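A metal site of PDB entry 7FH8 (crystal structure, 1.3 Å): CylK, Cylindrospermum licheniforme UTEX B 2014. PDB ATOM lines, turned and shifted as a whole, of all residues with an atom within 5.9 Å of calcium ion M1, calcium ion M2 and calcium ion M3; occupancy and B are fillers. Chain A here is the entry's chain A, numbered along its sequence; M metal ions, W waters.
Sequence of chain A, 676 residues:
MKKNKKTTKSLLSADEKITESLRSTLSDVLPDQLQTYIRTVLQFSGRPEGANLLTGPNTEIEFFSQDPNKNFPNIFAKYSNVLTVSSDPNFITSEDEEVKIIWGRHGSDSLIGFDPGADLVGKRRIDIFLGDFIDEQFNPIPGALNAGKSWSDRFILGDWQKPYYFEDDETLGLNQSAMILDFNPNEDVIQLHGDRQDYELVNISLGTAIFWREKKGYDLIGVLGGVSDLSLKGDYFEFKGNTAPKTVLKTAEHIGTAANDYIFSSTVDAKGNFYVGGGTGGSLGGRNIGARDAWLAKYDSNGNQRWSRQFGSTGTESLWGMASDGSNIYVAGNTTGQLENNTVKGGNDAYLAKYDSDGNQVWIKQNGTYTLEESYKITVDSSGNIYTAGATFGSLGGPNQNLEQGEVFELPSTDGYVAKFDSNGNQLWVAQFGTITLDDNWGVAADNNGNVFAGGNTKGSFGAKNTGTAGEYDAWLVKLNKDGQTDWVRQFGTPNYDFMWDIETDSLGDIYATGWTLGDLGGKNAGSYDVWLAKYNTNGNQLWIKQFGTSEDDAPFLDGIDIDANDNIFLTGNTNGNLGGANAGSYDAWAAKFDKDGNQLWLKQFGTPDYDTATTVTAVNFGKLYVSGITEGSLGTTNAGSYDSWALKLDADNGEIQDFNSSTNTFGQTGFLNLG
Calcium ion M1 is bound by the backbone carbonyl oxygen of Trp 151, the side-chain carboxylate of Asp 153, water W1, the side-chain carboxylate of Asp 132, the side-chain carboxylate of Glu 187 and the side-chain carboxylate of Asp 188.
Calcium ion M3 is bound by the backbone carbonyl oxygen of Ser 86 (2.3 Å), the backbone carbonyl oxygen of His 106 (2.3 Å), the backbone carbonyl oxygen of Gly 104 (2.3 Å), the backbone carbonyl oxygen of Thr 84 (2.4 Å), the side-chain carboxylate of Asp 88 (2.4 Å) and the side-chain carboxylate of Asp 109 (2.4 Å).
Calcium ion M3 has six donor atoms within binding distance.
Slightly farther from calcium ion M3 lies the side-chain carboxylate (OD2) of Asp 109 (3.1 Å).
Five residues have an atom within 4 Å of calcium ion M1: Asp 132, Trp 151, Asp 153, Glu 187 and Asp 188.
The nearest printed residue that does not touch calcium ion M1 is Ser 152 (4.4 Å).
The nearest printed residue that does not touch calcium ion M2 is Gly 104 (4.2 Å).
Calcium ion M2 is bound by OD2 of Asp 109 (2.3 Å), OD1 of Asp 132 (2.3 Å), O of Gly 131 (2.4 Å), OD1 of Asp 153 (2.4 Å), O of Gly 107 (2.4 Å) and O of Arg 105 (2.4 Å).
Water W1 bridges the side-chain carboxylate of Asp 188 and the side-chain carboxylate of Asp 182.
Seven residues have an atom within 4 Å of calcium ion M3: Thr 84, Ser 86, Asp 88, Gly 104, Arg 105, His 106 and Asp 109.
Along chain A the residues within 4 Å of calcium ion M3 span positions 84 to 109.
The backbone carbonyl oxygen of Leu 130 is in hydrogen-bond range of the backbone NH of Gly 104, 2.8 Å away.
N of Asp 132 is in hydrogen-bond range of OD2 of Asp 182, 2.9 Å away.
O of Asp 132 lies within hydrogen-bond range of NE1 of Trp 103 (3.0 Å).
OG of Ser 152 is in hydrogen-bond range of O of Glu 187, at 2.9 Å.
The side-chain hydroxyl (OG) of Ser 150 sits at hydrogen-bond distance from the side-chain carboxylate (OE1) of Glu 187, 2.6 Å away.
OD1 of Asp 182 is in hydrogen-bond range of N of Gly 131 (2.8 Å).
NH1 of Arg 105 is in hydrogen-bond range of O of Leu 83 (2.9 Å).
OD2 of Asp 188 sits at hydrogen-bond distance from N of Asn 184 (2.9 Å).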
ATOM      1  N   LEU A  83     -30.192  20.344  -4.513  1.00  0.00           N
ATOM      2  CA  LEU A  83     -30.219  19.495  -3.336  1.00  0.00           C
ATOM      3  C   LEU A  83     -28.895  19.612  -2.576  1.00  0.00           C
ATOM      4  O   LEU A  83     -28.119  20.546  -2.804  1.00  0.00           O
ATOM      5  CB  LEU A  83     -30.663  18.080  -3.721  1.00  0.00           C
ATOM      6  CG  LEU A  83     -32.096  18.072  -4.239  1.00  0.00           C
ATOM      7  CD1 LEU A  83     -32.431  16.738  -4.847  1.00  0.00           C
ATOM      8  CD2 LEU A  83     -33.062  18.384  -3.110  1.00  0.00           C
ATOM      9  N   THR A  84     -28.619  18.693  -1.648  1.00  0.00           N
ATOM     10  CA  THR A  84     -27.526  18.868  -0.692  1.00  0.00           C
ATOM     11  C   THR A  84     -26.380  17.911  -0.989  1.00  0.00           C
ATOM     12  O   THR A  84     -26.434  17.093  -1.914  1.00  0.00           O
ATOM     13  CB  THR A  84     -27.994  18.701   0.765  1.00  0.00           C
ATOM     14  OG1 THR A  84     -28.072  17.307   1.122  1.00  0.00           O
ATOM     15  CG2 THR A  84     -29.344  19.384   1.011  1.00  0.00           C
ATOM     16  N   VAL A  85     -25.335  18.004  -0.165  1.00  0.00           N
ATOM     17  CA  VAL A  85     -24.223  17.059  -0.242  1.00  0.00           C
ATOM     18  C   VAL A  85     -24.608  15.683   0.291  1.00  0.00           C
ATOM     19  O   VAL A  85     -23.851  14.729   0.125  1.00  0.00           O
ATOM     20  CB  VAL A  85     -22.986  17.703   0.424  1.00  0.00           C
ATOM     21  CG1 VAL A  85     -21.750  16.832   0.268  1.00  0.00           C
ATOM     22  CG2 VAL A  85     -22.716  19.087  -0.148  1.00  0.00           C
ATOM     23  N   SER A  86     -25.774  15.564   0.921  1.00  0.00           N
ATOM     24  CA  SER A  86     -26.288  14.314   1.459  1.00  0.00           C
ATOM     25  C   SER A  86     -26.885  13.458   0.356  1.00  0.00           C
ATOM     26  O   SER A  86     -27.101  13.905  -0.775  1.00  0.00           O
ATOM     27  CB  SER A  86     -27.429  14.581   2.448  1.00  0.00           C
ATOM     28  OG  SER A  86     -27.162  15.721   3.249  1.00  0.00           O
ATOM     29  N   SER A  87     -27.206  12.205   0.701  1.00  0.00           N
ATOM     30  CA  SER A  87     -28.013  11.360  -0.174  1.00  0.00           C
ATOM     31  C   SER A  87     -29.472  11.768   0.014  1.00  0.00           C
ATOM     32  O   SER A  87     -30.105  11.426   1.012  1.00  0.00           O
ATOM     33  CB  SER A  87     -27.797   9.891   0.167  1.00  0.00           C
ATOM     34  OG  SER A  87     -26.440   9.560  -0.062  1.00  0.00           O
ATOM     35  N   ASP A  88     -29.995  12.538  -0.950  1.00  0.00           N
ATOM     36  CA  ASP A  88     -31.258  13.258  -0.770  1.00  0.00           C
ATOM     37  C   ASP A  88     -32.407  12.580  -1.504  1.00  0.00           C
ATOM     38  O   ASP A  88     -32.292  12.265  -2.692  1.00  0.00           O
ATOM     39  CB  ASP A  88     -31.161  14.658  -1.400  1.00  0.00           C
ATOM     40  CG  ASP A  88     -30.059  15.509  -0.821  1.00  0.00           C
ATOM     41  OD1 ASP A  88     -30.115  15.804   0.399  1.00  0.00           O
ATOM     42  OD2 ASP A  88     -29.161  15.916  -1.584  1.00  0.00           O
ATOM     43  N   TRP A 103     -30.900  19.060  -9.269  1.00  0.00           N
ATOM     44  CA  TRP A 103     -29.456  18.866  -9.162  1.00  0.00           C
ATOM     45  C   TRP A 103     -29.156  18.137  -7.850  1.00  0.00           C
ATOM     46  O   TRP A 103     -29.238  18.713  -6.769  1.00  0.00           O
ATOM     47  CB  TRP A 103     -28.759  20.218  -9.234  1.00  0.00           C
ATOM     48  CG  TRP A 103     -27.269  20.171  -9.232  1.00  0.00           C
ATOM     49  CD1 TRP A 103     -26.473  19.107  -9.551  1.00  0.00           C
ATOM     50  CD2 TRP A 103     -26.385  21.234  -8.886  1.00  0.00           C
ATOM     51  NE1 TRP A 103     -25.144  19.453  -9.439  1.00  0.00           N
ATOM     52  CE2 TRP A 103     -25.070  20.759  -9.040  1.00  0.00           C
ATOM     53  CE3 TRP A 103     -26.583  22.561  -8.462  1.00  0.00           C
ATOM     54  CZ2 TRP A 103     -23.956  21.549  -8.763  1.00  0.00           C
ATOM     55  CZ3 TRP A 103     -25.472  23.331  -8.188  1.00  0.00           C
ATOM     56  CH2 TRP A 103     -24.174  22.827  -8.341  1.00  0.00           C
ATOM     57  N   GLY A 104     -28.784  16.849  -7.962  1.00  0.00           N
ATOM     58  CA  GLY A 104     -28.585  16.042  -6.764  1.00  0.00           C
ATOM     59  C   GLY A 104     -27.310  16.347  -6.001  1.00  0.00           C
ATOM     60  O   GLY A 104     -27.274  16.215  -4.772  1.00  0.00           O
ATOM     61  N   ARG A 105     -26.252  16.749  -6.700  1.00  0.00           N
ATOM     62  CA  ARG A 105     -24.929  16.942  -6.086  1.00  0.00           C
ATOM     63  C   ARG A 105     -24.447  15.634  -5.460  1.00  0.00           C
ATOM     64  O   ARG A 105     -24.828  14.541  -5.901  1.00  0.00           O
ATOM     65  CB  ARG A 105     -24.886  18.181  -5.196  1.00  0.00           C
ATOM     66  CG  ARG A 105     -25.116  19.464  -5.983  1.00  0.00           C
ATOM     67  CD  ARG A 105     -25.348  20.664  -5.083  1.00  0.00           C
ATOM     68  NE  ARG A 105     -24.196  21.040  -4.280  1.00  0.00           N
ATOM     69  CZ  ARG A 105     -24.243  21.410  -3.008  1.00  0.00           C
ATOM     70  NH1 ARG A 105     -25.387  21.416  -2.338  1.00  0.00           N
ATOM     71  NH2 ARG A 105     -23.120  21.810  -2.402  1.00  0.00           N
ATOM     72  N   HIS A 106     -23.601  15.720  -4.435  1.00  0.00           N
ATOM     73  CA  HIS A 106     -23.009  14.527  -3.870  1.00  0.00           C
ATOM     74  C   HIS A 106     -24.079  13.648  -3.242  1.00  0.00           C
ATOM     75  O   HIS A 106     -25.203  14.078  -2.964  1.00  0.00           O
ATOM     76  CB  HIS A 106     -21.999  14.891  -2.781  1.00  0.00           C
ATOM     77  CG  HIS A 106     -21.117  16.047  -3.136  1.00  0.00           C
ATOM     78  ND1 HIS A 106     -21.612  17.328  -3.293  1.00  0.00           N
ATOM     79  CD2 HIS A 106     -19.783  16.131  -3.337  1.00  0.00           C
ATOM     80  CE1 HIS A 106     -20.615  18.140  -3.590  1.00  0.00           C
ATOM     81  NE2 HIS A 106     -19.496  17.443  -3.620  1.00  0.00           N
ATOM     82  N   GLY A 107     -23.709  12.393  -2.991  1.00  0.00           N
ATOM     83  CA  GLY A 107     -24.615  11.455  -2.368  1.00  0.00           C
ATOM     84  C   GLY A 107     -25.442  10.677  -3.376  1.00  0.00           C
ATOM     85  O   GLY A 107     -25.528  11.002  -4.556  1.00  0.00           O
ATOM     86  N   SER A 108     -26.069   9.605  -2.869  1.00  0.00           N
ATOM     87  CA  SER A 108     -26.889   8.704  -3.674  1.00  0.00           C
ATOM     88  C   SER A 108     -28.321   9.234  -3.625  1.00  0.00           C
ATOM     89  O   SER A 108     -29.087   8.937  -2.708  1.00  0.00           O
ATOM     90  CB  SER A 108     -26.823   7.299  -3.093  1.00  0.00           C
ATOM     91  OG  SER A 108     -25.477   6.849  -3.037  1.00  0.00           O
ATOM     92  N   ASP A 109     -28.681  10.047  -4.603  1.00  0.00           N
ATOM     93  CA  ASP A 109     -29.925  10.797  -4.536  1.00  0.00           C
ATOM     94  C   ASP A 109     -31.081  10.040  -5.175  1.00  0.00           C
ATOM     95  O   ASP A 109     -30.907   9.311  -6.155  1.00  0.00           O
ATOM     96  CB  ASP A 109     -29.768  12.164  -5.203  1.00  0.00           C
ATOM     97  CG  ASP A 109     -28.628  12.965  -4.583  1.00  0.00           C
ATOM     98  OD1 ASP A 109     -28.730  13.287  -3.376  1.00  0.00           O
ATOM     99  OD2 ASP A 109     -27.621  13.240  -5.270  1.00  0.00           O
ATOM    100  N   LEU A 130     -29.668  16.254 -13.001  1.00  0.00           N
ATOM    101  CA  LEU A 130     -28.236  16.013 -12.822  1.00  0.00           C
ATOM    102  C   LEU A 130     -28.091  15.185 -11.552  1.00  0.00           C
ATOM    103  O   LEU A 130     -28.305  15.683 -10.443  1.00  0.00           O
ATOM    104  CB  LEU A 130     -27.474  17.337 -12.701  1.00  0.00           C
ATOM    105  CG  LEU A 130     -27.468  18.217 -13.958  1.00  0.00           C
ATOM    106  CD1 LEU A 130     -27.214  19.665 -13.571  1.00  0.00           C
ATOM    107  CD2 LEU A 130     -26.387  17.730 -14.907  1.00  0.00           C
ATOM    108  N   GLY A 131     -27.739  13.904 -11.710  1.00  0.00           N
ATOM    109  CA  GLY A 131     -27.628  13.040 -10.538  1.00  0.00           C
ATOM    110  C   GLY A 131     -26.514  13.458  -9.606  1.00  0.00           C
ATOM    111  O   GLY A 131     -26.675  13.482  -8.386  1.00  0.00           O
ATOM    112  N   ASP A 132     -25.343  13.772 -10.181  1.00  0.00           N
ATOM    113  CA  ASP A 132     -24.201  14.213  -9.403  1.00  0.00           C
ATOM    114  C   ASP A 132     -23.788  15.608  -9.853  1.00  0.00           C
ATOM    115  O   ASP A 132     -24.287  16.592  -9.298  1.00  0.00           O
ATOM    116  CB  ASP A 132     -23.052  13.196  -9.509  1.00  0.00           C
ATOM    117  CG  ASP A 132     -23.320  11.929  -8.705  1.00  0.00           C
ATOM    118  OD1 ASP A 132     -23.817  12.031  -7.559  1.00  0.00           O
ATOM    119  OD2 ASP A 132     -23.049  10.816  -9.217  1.00  0.00           O
ATOM    120  N   ILE A 134     -20.979  17.216  -9.373  1.00  0.00           N
ATOM    121  CA  ILE A 134     -20.656  17.749  -8.055  1.00  0.00           C
ATOM    122  C   ILE A 134     -19.828  19.026  -8.139  1.00  0.00           C
ATOM    123  O   ILE A 134     -19.202  19.340  -9.153  1.00  0.00           O
ATOM    124  CB  ILE A 134     -19.991  16.695  -7.150  1.00  0.00           C
ATOM    125  CG1 ILE A 134     -18.596  16.340  -7.677  1.00  0.00           C
ATOM    126  CG2 ILE A 134     -20.909  15.471  -6.987  1.00  0.00           C
ATOM    127  CD1 ILE A 134     -17.833  15.385  -6.772  1.00  0.00           C
ATOM    128  N   SER A 150     -18.344   9.842  -7.700  1.00  0.00           N
ATOM    129  CA  SER A 150     -19.753   9.870  -8.101  1.00  0.00           C
ATOM    130  C   SER A 150     -20.503   8.832  -7.285  1.00  0.00           C
ATOM    131  O   SER A 150     -19.901   8.000  -6.598  1.00  0.00           O
ATOM    132  CB  SER A 150     -19.913   9.641  -9.604  1.00  0.00           C
ATOM    133  OG  SER A 150     -19.325   8.417  -9.996  1.00  0.00           O
ATOM    134  N   TRP A 151     -21.833   8.889  -7.371  1.00  0.00           N
ATOM    135  CA  TRP A 151     -22.702   8.066  -6.541  1.00  0.00           C
ATOM    136  C   TRP A 151     -23.791   7.456  -7.410  1.00  0.00           C
ATOM    137  O   TRP A 151     -24.094   7.940  -8.496  1.00  0.00           O
ATOM    138  CB  TRP A 151     -23.364   8.912  -5.443  1.00  0.00           C
ATOM    139  CG  TRP A 151     -22.442   9.260  -4.300  1.00  0.00           C
ATOM    140  CD1 TRP A 151     -22.341   8.617  -3.102  1.00  0.00           C
ATOM    141  CD2 TRP A 151     -21.471  10.325  -4.270  1.00  0.00           C
ATOM    142  NE1 TRP A 151     -21.377   9.220  -2.323  1.00  0.00           N
ATOM    143  CE2 TRP A 151     -20.827  10.260  -3.019  1.00  0.00           C
ATOM    144  CE3 TRP A 151     -21.093  11.326  -5.174  1.00  0.00           C
ATOM    145  CZ2 TRP A 151     -19.825  11.154  -2.651  1.00  0.00           C
ATOM    146  CZ3 TRP A 151     -20.088  12.201  -4.816  1.00  0.00           C
ATOM    147  CH2 TRP A 151     -19.465  12.117  -3.555  1.00  0.00           C
ATOM    148  N   SER A 152     -24.404   6.384  -6.908  1.00  0.00           N
ATOM    149  CA  SER A 152     -25.575   5.801  -7.547  1.00  0.00           C
ATOM    150  C   SER A 152     -26.790   6.677  -7.278  1.00  0.00           C
ATOM    151  O   SER A 152     -27.278   6.739  -6.140  1.00  0.00           O
ATOM    152  CB  SER A 152     -25.802   4.394  -6.999  1.00  0.00           C
ATOM    153  OG  SER A 152     -24.720   3.536  -7.293  1.00  0.00           O
ATOM    154  N   ASP A 153     -27.296   7.351  -8.305  1.00  0.00           N
ATOM    155  CA  ASP A 153     -28.505   8.134  -8.207  1.00  0.00           C
ATOM    156  C   ASP A 153     -29.638   7.378  -8.890  1.00  0.00           C
ATOM    157  O   ASP A 153     -29.410   6.652  -9.864  1.00  0.00           O
ATOM    158  CB  ASP A 153     -28.340   9.499  -8.870  1.00  0.00           C
ATOM    159  CG  ASP A 153     -27.156  10.243  -8.330  1.00  0.00           C
ATOM    160  OD1 ASP A 153     -27.211  10.642  -7.141  1.00  0.00           O
ATOM    161  OD2 ASP A 153     -26.164  10.423  -9.063  1.00  0.00           O
ATOM    162  N   PHE A 155     -33.139   7.958 -10.822  1.00  0.00           N
ATOM    163  CA  PHE A 155     -33.924   8.947 -11.544  1.00  0.00           C
ATOM    164  C   PHE A 155     -35.329   8.371 -11.696  1.00  0.00           C
ATOM    165  O   PHE A 155     -35.520   7.362 -12.383  1.00  0.00           O
ATOM    166  CB  PHE A 155     -33.318   9.259 -12.910  1.00  0.00           C
ATOM    167  CG  PHE A 155     -31.901   9.772 -12.845  1.00  0.00           C
ATOM    168  CD1 PHE A 155     -31.643  11.121 -12.585  1.00  0.00           C
ATOM    169  CD2 PHE A 155     -30.824   8.926 -13.062  1.00  0.00           C
ATOM    170  CE1 PHE A 155     -30.346  11.599 -12.541  1.00  0.00           C
ATOM    171  CE2 PHE A 155     -29.514   9.403 -13.022  1.00  0.00           C
ATOM    172  CZ  PHE A 155     -29.279  10.745 -12.763  1.00  0.00           C
ATOM    173  N   ASP A 182     -26.552  13.331 -17.000  1.00  0.00           N
ATOM    174  CA  ASP A 182     -25.330  12.671 -16.541  1.00  0.00           C
ATOM    175  C   ASP A 182     -25.608  11.233 -16.123  1.00  0.00           C
ATOM    176  O   ASP A 182     -25.013  10.718 -15.167  1.00  0.00           O
ATOM    177  CB  ASP A 182     -24.669  13.435 -15.396  1.00  0.00           C
ATOM    178  CG  ASP A 182     -25.461  13.354 -14.098  1.00  0.00           C
ATOM    179  OD1 ASP A 182     -26.708  13.280 -14.190  1.00  0.00           O
ATOM    180  OD2 ASP A 182     -24.854  13.339 -13.001  1.00  0.00           O
ATOM    181  N   ASN A 184     -25.125   7.561 -15.739  1.00  0.00           N
ATOM    182  CA  ASN A 184     -24.000   6.639 -15.854  1.00  0.00           C
ATOM    183  C   ASN A 184     -24.541   5.224 -15.644  1.00  0.00           C
ATOM    184  O   ASN A 184     -24.872   4.872 -14.507  1.00  0.00           O
ATOM    185  CB  ASN A 184     -22.939   6.970 -14.807  1.00  0.00           C
ATOM    186  CG  ASN A 184     -21.741   6.034 -14.872  1.00  0.00           C
ATOM    187  OD1 ASN A 184     -21.778   4.991 -15.512  1.00  0.00           O
ATOM    188  ND2 ASN A 184     -20.652   6.421 -14.205  1.00  0.00           N
ATOM    189  N   GLU A 187     -23.560   2.959 -12.620  1.00  0.00           N
ATOM    190  CA  GLU A 187     -23.847   3.304 -11.228  1.00  0.00           C
ATOM    191  C   GLU A 187     -25.314   3.690 -11.011  1.00  0.00           C
ATOM    192  O   GLU A 187     -25.897   3.319  -9.987  1.00  0.00           O
ATOM    193  CB  GLU A 187     -22.926   4.439 -10.734  1.00  0.00           C
ATOM    194  CG  GLU A 187     -23.100   5.772 -11.478  1.00  0.00           C
ATOM    195  CD  GLU A 187     -22.272   6.930 -10.909  1.00  0.00           C
ATOM    196  OE1 GLU A 187     -21.209   6.659 -10.304  1.00  0.00           O
ATOM    197  OE2 GLU A 187     -22.680   8.109 -11.069  1.00  0.00           O
ATOM    198  N   ASP A 188     -25.897   4.453 -11.929  1.00  0.00           N
ATOM    199  CA  ASP A 188     -27.203   5.052 -11.708  1.00  0.00           C
ATOM    200  C   ASP A 188     -28.326   4.091 -12.087  1.00  0.00           C
ATOM    201  O   ASP A 188     -28.104   3.071 -12.758  1.00  0.00           O
ATOM    202  CB  ASP A 188     -27.360   6.332 -12.547  1.00  0.00           C
ATOM    203  CG  ASP A 188     -26.391   7.431 -12.154  1.00  0.00           C
ATOM    204  OD1 ASP A 188     -26.052   7.591 -10.967  1.00  0.00           O
ATOM    205  OD2 ASP A 188     -25.963   8.173 -13.064  1.00  0.00           O
HETATM  206 CA    CA M   1     -24.533   9.308 -10.243  1.00  0.00          CA
HETATM  207 CA    CA M   2     -25.826  12.439  -6.440  1.00  0.00          CA
HETATM  208 CA    CA M   3     -27.295  15.065  -2.752  1.00  0.00          CA
HETATM  209  O   HOH W   1     -25.033  10.598 -12.140  1.00  0.00           O
